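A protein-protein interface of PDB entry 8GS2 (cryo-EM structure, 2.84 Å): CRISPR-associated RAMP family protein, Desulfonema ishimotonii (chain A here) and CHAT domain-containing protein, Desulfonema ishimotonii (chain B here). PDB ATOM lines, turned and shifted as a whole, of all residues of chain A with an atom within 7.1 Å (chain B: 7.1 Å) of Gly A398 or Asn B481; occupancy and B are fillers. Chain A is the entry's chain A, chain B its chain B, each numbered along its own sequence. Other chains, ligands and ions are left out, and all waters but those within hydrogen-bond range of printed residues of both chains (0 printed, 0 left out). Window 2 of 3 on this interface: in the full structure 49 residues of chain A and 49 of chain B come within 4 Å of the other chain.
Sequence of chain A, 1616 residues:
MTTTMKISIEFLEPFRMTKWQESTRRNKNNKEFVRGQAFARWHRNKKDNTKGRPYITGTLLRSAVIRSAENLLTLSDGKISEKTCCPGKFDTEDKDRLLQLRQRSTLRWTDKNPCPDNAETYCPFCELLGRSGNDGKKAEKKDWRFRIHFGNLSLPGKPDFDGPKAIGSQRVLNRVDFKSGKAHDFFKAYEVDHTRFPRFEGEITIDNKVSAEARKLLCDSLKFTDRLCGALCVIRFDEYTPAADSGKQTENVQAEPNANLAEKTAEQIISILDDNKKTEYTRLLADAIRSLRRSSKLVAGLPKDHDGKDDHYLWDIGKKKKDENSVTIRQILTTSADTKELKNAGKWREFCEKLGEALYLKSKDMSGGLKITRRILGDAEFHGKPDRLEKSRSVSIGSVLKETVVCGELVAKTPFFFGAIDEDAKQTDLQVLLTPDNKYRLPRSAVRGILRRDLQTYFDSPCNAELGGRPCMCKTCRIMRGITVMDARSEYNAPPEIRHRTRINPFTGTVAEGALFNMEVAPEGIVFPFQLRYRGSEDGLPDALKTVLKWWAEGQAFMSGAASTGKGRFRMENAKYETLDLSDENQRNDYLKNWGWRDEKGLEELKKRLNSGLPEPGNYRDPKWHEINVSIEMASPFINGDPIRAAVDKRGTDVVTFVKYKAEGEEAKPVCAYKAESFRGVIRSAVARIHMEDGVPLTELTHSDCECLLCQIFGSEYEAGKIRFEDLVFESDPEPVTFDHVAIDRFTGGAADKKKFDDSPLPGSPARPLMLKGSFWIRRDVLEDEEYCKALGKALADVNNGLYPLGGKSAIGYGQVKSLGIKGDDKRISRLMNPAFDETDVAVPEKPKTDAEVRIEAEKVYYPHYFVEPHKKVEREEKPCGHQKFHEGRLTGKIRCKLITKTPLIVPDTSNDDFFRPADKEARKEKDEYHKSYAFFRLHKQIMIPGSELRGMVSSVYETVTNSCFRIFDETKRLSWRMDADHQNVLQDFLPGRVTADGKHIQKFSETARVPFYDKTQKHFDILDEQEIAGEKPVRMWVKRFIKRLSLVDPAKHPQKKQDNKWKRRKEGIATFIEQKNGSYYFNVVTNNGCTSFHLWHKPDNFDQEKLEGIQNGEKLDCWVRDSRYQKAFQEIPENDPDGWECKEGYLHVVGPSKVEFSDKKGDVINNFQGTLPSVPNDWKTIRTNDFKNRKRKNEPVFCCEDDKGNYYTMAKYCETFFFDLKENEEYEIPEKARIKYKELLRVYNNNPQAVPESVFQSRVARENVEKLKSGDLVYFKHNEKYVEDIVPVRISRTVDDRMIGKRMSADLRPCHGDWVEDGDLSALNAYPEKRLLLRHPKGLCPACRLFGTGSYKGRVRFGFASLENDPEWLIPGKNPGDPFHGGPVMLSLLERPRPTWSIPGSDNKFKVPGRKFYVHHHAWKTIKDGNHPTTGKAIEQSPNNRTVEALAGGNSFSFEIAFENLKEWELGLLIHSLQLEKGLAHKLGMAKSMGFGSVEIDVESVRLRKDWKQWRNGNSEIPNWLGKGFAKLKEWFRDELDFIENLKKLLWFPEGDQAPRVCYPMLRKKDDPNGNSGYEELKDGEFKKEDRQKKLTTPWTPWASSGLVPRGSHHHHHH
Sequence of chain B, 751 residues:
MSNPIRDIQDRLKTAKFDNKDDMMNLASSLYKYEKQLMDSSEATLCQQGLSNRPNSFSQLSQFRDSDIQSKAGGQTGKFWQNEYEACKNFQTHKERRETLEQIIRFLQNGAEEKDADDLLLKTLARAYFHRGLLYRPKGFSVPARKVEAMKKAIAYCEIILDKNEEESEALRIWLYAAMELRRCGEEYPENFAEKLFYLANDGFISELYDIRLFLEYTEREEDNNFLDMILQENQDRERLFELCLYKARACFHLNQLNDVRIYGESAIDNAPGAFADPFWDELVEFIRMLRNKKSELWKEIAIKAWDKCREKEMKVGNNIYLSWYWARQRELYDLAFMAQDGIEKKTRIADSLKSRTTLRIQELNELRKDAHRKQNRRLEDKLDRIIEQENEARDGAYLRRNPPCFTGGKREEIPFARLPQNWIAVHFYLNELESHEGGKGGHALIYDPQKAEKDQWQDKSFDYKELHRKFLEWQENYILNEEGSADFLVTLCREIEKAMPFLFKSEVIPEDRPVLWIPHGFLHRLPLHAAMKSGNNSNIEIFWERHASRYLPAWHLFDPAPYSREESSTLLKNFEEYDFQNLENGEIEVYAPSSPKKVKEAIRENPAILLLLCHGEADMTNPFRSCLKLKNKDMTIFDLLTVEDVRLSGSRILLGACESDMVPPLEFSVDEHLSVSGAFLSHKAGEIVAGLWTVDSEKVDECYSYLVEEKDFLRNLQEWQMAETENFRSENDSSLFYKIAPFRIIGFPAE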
ATOM      1  N   ASN A  71      17.137 -25.293  -4.235  1.00  0.00           N
ATOM      2  CA  ASN A  71      17.883 -24.980  -5.452  1.00  0.00           C
ATOM      3  C   ASN A  71      17.654 -23.536  -5.893  1.00  0.00           C
ATOM      4  O   ASN A  71      18.607 -22.828  -6.246  1.00  0.00           O
ATOM      5  CB  ASN A  71      17.500 -25.948  -6.571  1.00  0.00           C
ATOM      6  CG  ASN A  71      18.086 -27.331  -6.372  1.00  0.00           C
ATOM      7  OD1 ASN A  71      17.360 -28.302  -6.160  1.00  0.00           O
ATOM      8  ND2 ASN A  71      19.407 -27.428  -6.445  1.00  0.00           N
ATOM      9  N   THR A  74      19.418 -21.122  -3.624  1.00  0.00           N
ATOM     10  CA  THR A  74      20.840 -21.136  -3.944  1.00  0.00           C
ATOM     11  C   THR A  74      21.127 -20.302  -5.188  1.00  0.00           C
ATOM     12  O   THR A  74      22.135 -19.590  -5.247  1.00  0.00           O
ATOM     13  CB  THR A  74      21.322 -22.573  -4.134  1.00  0.00           C
ATOM     14  OG1 THR A  74      21.028 -23.331  -2.955  1.00  0.00           O
ATOM     15  CG2 THR A  74      22.817 -22.604  -4.383  1.00  0.00           C
ATOM     16  N   LEU A  75      20.247 -20.376  -6.190  1.00  0.00           N
ATOM     17  CA  LEU A  75      20.443 -19.589  -7.405  1.00  0.00           C
ATOM     18  C   LEU A  75      20.363 -18.091  -7.131  1.00  0.00           C
ATOM     19  O   LEU A  75      21.164 -17.315  -7.664  1.00  0.00           O
ATOM     20  CB  LEU A  75      19.416 -19.988  -8.463  1.00  0.00           C
ATOM     21  CG  LEU A  75      19.587 -21.377  -9.073  1.00  0.00           C
ATOM     22  CD1 LEU A  75      18.579 -21.600 -10.184  1.00  0.00           C
ATOM     23  CD2 LEU A  75      21.001 -21.543  -9.586  1.00  0.00           C
ATOM     24  N   ASP A  77      20.843 -16.323  -4.333  1.00  0.00           N
ATOM     25  CA  ASP A  77      21.567 -15.875  -3.141  1.00  0.00           C
ATOM     26  C   ASP A  77      20.685 -15.879  -1.896  1.00  0.00           C
ATOM     27  O   ASP A  77      20.912 -15.108  -0.960  1.00  0.00           O
ATOM     28  CB  ASP A  77      22.180 -14.485  -3.350  1.00  0.00           C
ATOM     29  CG  ASP A  77      23.181 -14.455  -4.487  1.00  0.00           C
ATOM     30  OD1 ASP A  77      23.829 -15.492  -4.738  1.00  0.00           O
ATOM     31  OD2 ASP A  77      23.320 -13.392  -5.127  1.00  0.00           O
ATOM     32  N   LEU A 107      21.558 -27.676   0.759  1.00  0.00           N
ATOM     33  CA  LEU A 107      22.175 -26.555   0.066  1.00  0.00           C
ATOM     34  C   LEU A 107      22.232 -25.334   0.976  1.00  0.00           C
ATOM     35  O   LEU A 107      21.320 -25.085   1.769  1.00  0.00           O
ATOM     36  CB  LEU A 107      21.405 -26.229  -1.214  1.00  0.00           C
ATOM     37  CG  LEU A 107      21.775 -27.008  -2.481  1.00  0.00           C
ATOM     38  CD1 LEU A 107      21.537 -28.499  -2.324  1.00  0.00           C
ATOM     39  CD2 LEU A 107      21.000 -26.478  -3.669  1.00  0.00           C
ATOM     40  N   ARG A 108      23.317 -24.574   0.862  1.00  0.00           N
ATOM     41  CA  ARG A 108      23.545 -23.397   1.686  1.00  0.00           C
ATOM     42  C   ARG A 108      23.539 -22.141   0.826  1.00  0.00           C
ATOM     43  O   ARG A 108      24.140 -22.111  -0.252  1.00  0.00           O
ATOM     44  CB  ARG A 108      24.873 -23.501   2.442  1.00  0.00           C
ATOM     45  CG  ARG A 108      25.260 -22.226   3.173  1.00  0.00           C
ATOM     46  CD  ARG A 108      26.604 -22.347   3.867  1.00  0.00           C
ATOM     47  NE  ARG A 108      26.556 -23.254   5.006  1.00  0.00           N
ATOM     48  CZ  ARG A 108      27.501 -23.337   5.933  1.00  0.00           C
ATOM     49  NH1 ARG A 108      28.579 -22.572   5.892  1.00  0.00           N
ATOM     50  NH2 ARG A 108      27.359 -24.208   6.928  1.00  0.00           N
ATOM     51  N   VAL A 395      26.083 -27.903   2.634  1.00  0.00           N
ATOM     52  CA  VAL A 395      27.103 -27.763   1.602  1.00  0.00           C
ATOM     53  C   VAL A 395      26.649 -26.692   0.621  1.00  0.00           C
ATOM     54  O   VAL A 395      25.501 -26.708   0.164  1.00  0.00           O
ATOM     55  CB  VAL A 395      27.364 -29.093   0.869  1.00  0.00           C
ATOM     56  CG1 VAL A 395      28.291 -28.876  -0.312  1.00  0.00           C
ATOM     57  CG2 VAL A 395      27.957 -30.114   1.824  1.00  0.00           C
ATOM     58  N   SER A 396      27.547 -25.765   0.298  1.00  0.00           N
ATOM     59  CA  SER A 396      27.276 -24.706  -0.664  1.00  0.00           C
ATOM     60  C   SER A 396      27.816 -25.111  -2.029  1.00  0.00           C
ATOM     61  O   SER A 396      28.981 -25.502  -2.149  1.00  0.00           O
ATOM     62  CB  SER A 396      27.907 -23.386  -0.217  1.00  0.00           C
ATOM     63  OG  SER A 396      27.685 -22.367  -1.173  1.00  0.00           O
ATOM     64  N   ILE A 397      26.966 -25.018  -3.055  1.00  0.00           N
ATOM     65  CA  ILE A 397      27.341 -25.417  -4.406  1.00  0.00           C
ATOM     66  C   ILE A 397      27.585 -24.227  -5.321  1.00  0.00           C
ATOM     67  O   ILE A 397      27.919 -24.421  -6.497  1.00  0.00           O
ATOM     68  CB  ILE A 397      26.280 -26.348  -5.024  1.00  0.00           C
ATOM     69  CG1 ILE A 397      24.955 -25.605  -5.196  1.00  0.00           C
ATOM     70  CG2 ILE A 397      26.091 -27.584  -4.163  1.00  0.00           C
ATOM     71  CD1 ILE A 397      23.900 -26.408  -5.916  1.00  0.00           C
ATOM     72  N   GLY A 398      27.429 -23.005  -4.822  1.00  0.00           N
ATOM     73  CA  GLY A 398      27.644 -21.819  -5.621  1.00  0.00           C
ATOM     74  C   GLY A 398      26.392 -21.367  -6.351  1.00  0.00           C
ATOM     75  O   GLY A 398      25.374 -22.059  -6.415  1.00  0.00           O
ATOM     76  N   SER A 399      26.481 -20.166  -6.916  1.00  0.00           N
ATOM     77  CA  SER A 399      25.368 -19.558  -7.632  1.00  0.00           C
ATOM     78  C   SER A 399      25.421 -19.795  -9.135  1.00  0.00           C
ATOM     79  O   SER A 399      24.571 -19.266  -9.859  1.00  0.00           O
ATOM     80  CB  SER A 399      25.324 -18.052  -7.354  1.00  0.00           C
ATOM     81  OG  SER A 399      24.296 -17.430  -8.104  1.00  0.00           O
ATOM     82  N   VAL A 400      26.388 -20.568  -9.621  1.00  0.00           N
ATOM     83  CA  VAL A 400      26.545 -20.836 -11.045  1.00  0.00           C
ATOM     84  C   VAL A 400      25.879 -22.167 -11.356  1.00  0.00           C
ATOM     85  O   VAL A 400      26.278 -23.209 -10.823  1.00  0.00           O
ATOM     86  CB  VAL A 400      28.026 -20.851 -11.453  1.00  0.00           C
ATOM     87  CG1 VAL A 400      28.165 -21.188 -12.929  1.00  0.00           C
ATOM     88  CG2 VAL A 400      28.678 -19.513 -11.141  1.00  0.00           C
ATOM     89  N   LEU A 401      24.866 -22.137 -12.219  1.00  0.00           N
ATOM     90  CA  LEU A 401      24.153 -23.342 -12.626  1.00  0.00           C
ATOM     91  C   LEU A 401      23.730 -23.188 -14.077  1.00  0.00           C
ATOM     92  O   LEU A 401      23.007 -22.246 -14.416  1.00  0.00           O
ATOM     93  CB  LEU A 401      22.931 -23.590 -11.737  1.00  0.00           C
ATOM     94  CG  LEU A 401      22.227 -24.938 -11.887  1.00  0.00           C
ATOM     95  CD1 LEU A 401      23.066 -26.044 -11.270  1.00  0.00           C
ATOM     96  CD2 LEU A 401      20.841 -24.894 -11.262  1.00  0.00           C
ATOM     97  N   SER A 537      27.430 -26.863 -12.648  1.00  0.00           N
ATOM     98  CA  SER A 537      28.126 -25.589 -12.550  1.00  0.00           C
ATOM     99  C   SER A 537      29.168 -25.391 -13.643  1.00  0.00           C
ATOM    100  O   SER A 537      29.787 -24.324 -13.700  1.00  0.00           O
ATOM    101  CB  SER A 537      28.791 -25.457 -11.176  1.00  0.00           C
ATOM    102  OG  SER A 537      29.719 -26.503 -10.956  1.00  0.00           O
ATOM    103  N   SER A 583      21.566 -19.165 -13.961  1.00  0.00           N
ATOM    104  CA  SER A 583      21.975 -18.150 -12.998  1.00  0.00           C
ATOM    105  C   SER A 583      21.382 -16.787 -13.328  1.00  0.00           C
ATOM    106  O   SER A 583      21.053 -16.020 -12.417  1.00  0.00           O
ATOM    107  CB  SER A 583      23.499 -18.062 -12.941  1.00  0.00           C
ATOM    108  OG  SER A 583      24.066 -19.316 -12.608  1.00  0.00           O
ATOM    109  N   TRP B 474      33.492 -29.982   5.270  1.00  0.00           N
ATOM    110  CA  TRP B 474      34.635 -29.430   4.550  1.00  0.00           C
ATOM    111  C   TRP B 474      35.047 -30.330   3.393  1.00  0.00           C
ATOM    112  O   TRP B 474      35.379 -29.840   2.308  1.00  0.00           O
ATOM    113  CB  TRP B 474      35.809 -29.217   5.504  1.00  0.00           C
ATOM    114  CG  TRP B 474      37.085 -28.904   4.791  1.00  0.00           C
ATOM    115  CD1 TRP B 474      37.502 -27.681   4.357  1.00  0.00           C
ATOM    116  CD2 TRP B 474      38.110 -29.833   4.420  1.00  0.00           C
ATOM    117  NE1 TRP B 474      38.724 -27.790   3.740  1.00  0.00           N
ATOM    118  CE2 TRP B 474      39.118 -29.101   3.765  1.00  0.00           C
ATOM    119  CE3 TRP B 474      38.271 -31.212   4.576  1.00  0.00           C
ATOM    120  CZ2 TRP B 474      40.273 -29.701   3.270  1.00  0.00           C
ATOM    121  CZ3 TRP B 474      39.416 -31.806   4.084  1.00  0.00           C
ATOM    122  CH2 TRP B 474      40.403 -31.052   3.439  1.00  0.00           C
ATOM    123  N   GLU B 476      33.225 -32.406   1.578  1.00  0.00           N
ATOM    124  CA  GLU B 476      32.291 -32.324   0.461  1.00  0.00           C
ATOM    125  C   GLU B 476      32.330 -30.950  -0.196  1.00  0.00           C
ATOM    126  O   GLU B 476      32.249 -30.843  -1.425  1.00  0.00           O
ATOM    127  CB  GLU B 476      30.878 -32.656   0.932  1.00  0.00           C
ATOM    128  CG  GLU B 476      29.859 -32.696  -0.188  1.00  0.00           C
ATOM    129  CD  GLU B 476      28.507 -33.186   0.277  1.00  0.00           C
ATOM    130  OE1 GLU B 476      28.371 -33.498   1.479  1.00  0.00           O
ATOM    131  OE2 GLU B 476      27.580 -33.258  -0.556  1.00  0.00           O
ATOM    132  N   ASN B 477      32.447 -29.887   0.603  1.00  0.00           N
ATOM    133  CA  ASN B 477      32.555 -28.548   0.035  1.00  0.00           C
ATOM    134  C   ASN B 477      33.837 -28.378  -0.765  1.00  0.00           C
ATOM    135  O   ASN B 477      33.845 -27.663  -1.773  1.00  0.00           O
ATOM    136  CB  ASN B 477      32.479 -27.494   1.138  1.00  0.00           C
ATOM    137  CG  ASN B 477      31.055 -27.134   1.502  1.00  0.00           C
ATOM    138  OD1 ASN B 477      30.460 -27.731   2.398  1.00  0.00           O
ATOM    139  ND2 ASN B 477      30.499 -26.151   0.806  1.00  0.00           N
ATOM    140  N   TYR B 478      34.926 -29.018  -0.334  1.00  0.00           N
ATOM    141  CA  TYR B 478      36.172 -28.947  -1.087  1.00  0.00           C
ATOM    142  C   TYR B 478      36.013 -29.562  -2.470  1.00  0.00           C
ATOM    143  O   TYR B 478      36.545 -29.041  -3.457  1.00  0.00           O
ATOM    144  CB  TYR B 478      37.290 -29.643  -0.310  1.00  0.00           C
ATOM    145  CG  TYR B 478      38.635 -29.613  -0.997  1.00  0.00           C
ATOM    146  CD1 TYR B 478      39.459 -28.500  -0.903  1.00  0.00           C
ATOM    147  CD2 TYR B 478      39.085 -30.700  -1.733  1.00  0.00           C
ATOM    148  CE1 TYR B 478      40.689 -28.468  -1.528  1.00  0.00           C
ATOM    149  CE2 TYR B 478      40.314 -30.677  -2.362  1.00  0.00           C
ATOM    150  CZ  TYR B 478      41.111 -29.559  -2.256  1.00  0.00           C
ATOM    151  OH  TYR B 478      42.336 -29.532  -2.880  1.00  0.00           O
ATOM    152  N   ILE B 479      35.284 -30.673  -2.562  1.00  0.00           N
ATOM    153  CA  ILE B 479      35.086 -31.336  -3.846  1.00  0.00           C
ATOM    154  C   ILE B 479      34.067 -30.586  -4.694  1.00  0.00           C
ATOM    155  O   ILE B 479      34.303 -30.309  -5.875  1.00  0.00           O
ATOM    156  CB  ILE B 479      34.667 -32.800  -3.623  1.00  0.00           C
ATOM    157  CG1 ILE B 479      35.744 -33.547  -2.836  1.00  0.00           C
ATOM    158  CG2 ILE B 479      34.398 -33.485  -4.948  1.00  0.00           C
ATOM    159  CD1 ILE B 479      35.399 -34.992  -2.549  1.00  0.00           C
ATOM    160  N   LEU B 480      32.917 -30.244  -4.107  1.00  0.00           N
ATOM    161  CA  LEU B 480      31.842 -29.636  -4.884  1.00  0.00           C
ATOM    162  C   LEU B 480      32.158 -28.194  -5.262  1.00  0.00           C
ATOM    163  O   LEU B 480      31.945 -27.790  -6.411  1.00  0.00           O
ATOM    164  CB  LEU B 480      30.528 -29.704  -4.108  1.00  0.00           C
ATOM    165  CG  LEU B 480      29.870 -31.077  -4.008  1.00  0.00           C
ATOM    166  CD1 LEU B 480      28.552 -30.981  -3.264  1.00  0.00           C
ATOM    167  CD2 LEU B 480      29.663 -31.669  -5.391  1.00  0.00           C
ATOM    168  N   ASN B 481      32.659 -27.403  -4.315  1.00  0.00           N
ATOM    169  CA  ASN B 481      32.848 -25.964  -4.511  1.00  0.00           C
ATOM    170  C   ASN B 481      34.254 -25.585  -4.059  1.00  0.00           C
ATOM    171  O   ASN B 481      34.465 -25.209  -2.903  1.00  0.00           O
ATOM    172  CB  ASN B 481      31.780 -25.177  -3.756  1.00  0.00           C
ATOM    173  CG  ASN B 481      31.903 -23.683  -3.959  1.00  0.00           C
ATOM    174  OD1 ASN B 481      32.551 -22.991  -3.176  1.00  0.00           O
ATOM    175  ND2 ASN B 481      31.277 -23.175  -5.013  1.00  0.00           N
ATOM    176  N   GLU B 482      35.211 -25.673  -4.978  1.00  0.00           N
ATOM    177  CA  GLU B 482      36.576 -25.271  -4.676  1.00  0.00           C
ATOM    178  C   GLU B 482      36.653 -23.759  -4.488  1.00  0.00           C
ATOM    179  O   GLU B 482      35.862 -22.999  -5.054  1.00  0.00           O
ATOM    180  CB  GLU B 482      37.521 -25.720  -5.794  1.00  0.00           C
ATOM    181  CG  GLU B 482      38.999 -25.511  -5.498  1.00  0.00           C
ATOM    182  CD  GLU B 482      39.468 -26.286  -4.283  1.00  0.00           C
ATOM    183  OE1 GLU B 482      38.917 -27.375  -4.020  1.00  0.00           O
ATOM    184  OE2 GLU B 482      40.387 -25.805  -3.589  1.00  0.00           O
ATOM    185  N   GLU B 483      37.609 -23.331  -3.661  1.00  0.00           N
ATOM    186  CA  GLU B 483      37.886 -21.940  -3.307  1.00  0.00           C
ATOM    187  C   GLU B 483      36.784 -21.317  -2.462  1.00  0.00           C
ATOM    188  O   GLU B 483      36.886 -20.135  -2.111  1.00  0.00           O
ATOM    189  CB  GLU B 483      38.133 -21.055  -4.538  1.00  0.00           C
ATOM    190  CG  GLU B 483      39.274 -21.527  -5.423  1.00  0.00           C
ATOM    191  CD  GLU B 483      38.831 -21.787  -6.849  1.00  0.00           C
ATOM    192  OE1 GLU B 483      37.613 -21.720  -7.116  1.00  0.00           O
ATOM    193  OE2 GLU B 483      39.702 -22.060  -7.703  1.00  0.00           O
ATOM    194  N   GLY B 484      35.733 -22.060  -2.126  1.00  0.00           N
ATOM    195  CA  GLY B 484      34.709 -21.571  -1.229  1.00  0.00           C
ATOM    196  C   GLY B 484      34.671 -22.365   0.059  1.00  0.00           C
ATOM    197  O   GLY B 484      33.854 -22.099   0.945  1.00  0.00           O
ATOM    198  N   SER B 485      35.560 -23.349   0.169  1.00  0.00           N
ATOM    199  CA  SER B 485      35.653 -24.198   1.348  1.00  0.00           C
ATOM    200  C   SER B 485      36.632 -23.667   2.384  1.00  0.00           C
ATOM    201  O   SER B 485      36.848 -24.326   3.406  1.00  0.00           O
ATOM    202  CB  SER B 485      36.055 -25.619   0.943  1.00  0.00           C
ATOM    203  OG  SER B 485      37.301 -25.623   0.268  1.00  0.00           O
ATOM    204  N   ALA B 486      37.235 -22.499   2.143  1.00  0.00           N
ATOM    205  CA  ALA B 486      38.131 -21.913   3.134  1.00  0.00           C
ATOM    206  C   ALA B 486      37.384 -21.577   4.416  1.00  0.00           C
ATOM    207  O   ALA B 486      37.928 -21.720   5.517  1.00  0.00           O
ATOM    208  CB  ALA B 486      38.808 -20.669   2.562  1.00  0.00           C
ATOM    209  N   PHE B 488      34.800 -23.227   5.605  1.00  0.00           N
ATOM    210  CA  PHE B 488      34.593 -24.490   6.306  1.00  0.00           C
ATOM    211  C   PHE B 488      35.880 -24.979   6.959  1.00  0.00           C
ATOM    212  O   PHE B 488      35.847 -25.541   8.061  1.00  0.00           O
ATOM    213  CB  PHE B 488      34.046 -25.541   5.343  1.00  0.00           C
ATOM    214  CG  PHE B 488      32.667 -25.234   4.832  1.00  0.00           C
ATOM    215  CD1 PHE B 488      32.490 -24.445   3.707  1.00  0.00           C
ATOM    216  CD2 PHE B 488      31.549 -25.731   5.477  1.00  0.00           C
ATOM    217  CE1 PHE B 488      31.224 -24.161   3.237  1.00  0.00           C
ATOM    218  CE2 PHE B 488      30.280 -25.450   5.010  1.00  0.00           C
ATOM    219  CZ  PHE B 488      30.118 -24.665   3.888  1.00  0.00           C
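The backbone NH of Ser A396 lies close to the side-chain amide nitrogen of Asn B477.
N of Arg A108 is in hydrogen-bond range of O of Val A395 (3.1 Å).
The backbone NH (N) of Gly B484 sits close to the side-chain amide oxygen (OD1) of Asn B481, at 3.5 Å.
Among the printed residues, pairs that only touch across the chains: Ser A396 with Asn B481, Arg A108 with Phe B488, Val A395 with Glu B476, Val A395 with Asn B477, Val A395 with Leu B480, Ile A397 with Asn B481 and Gly A398 with Asn B481.
Printed residues of chain B within 4 Å of Gly A398: Asn B481 (3.9 Å).
Of the printed residues of chain A, Leu B480 touches Val A395 (3.6 Å).
Of the printed residues of chain A, Glu B476 touches Val A395 (3.4 Å).
Of the printed residues of chain A, Phe B488 touches Arg A108.
Of the printed residues of chain B, Val A395 touches Glu B476 (3.4 Å), Asn B477 (3.5 Å) and Leu B480 (3.6 Å).
Of the printed residues of chain B, Ile A397 touches Asn B481.
Asp A77 touches none of the printed residues of chain B.
Leu A107 touches none of the printed residues of chain B.
The nearest printed residue of chain B that does not touch Ile A397 is Leu B480 (4.3 Å).
Printed residues of chain A that touch a printed residue of chain B: Arg A108, Val A395, Ser A396, Ile A397 and Gly A398.
Hydrophobic or aromatic side chains of chain B that line the printed part of chain A: Leu B480 and Phe B488.
Among the printed residues, 8 pairs touch across the chains.
Among the printed residues, no Asp or Glu carboxylate lies within 4 Å of a Lys or Arg side-chain nitrogen of the other chain.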
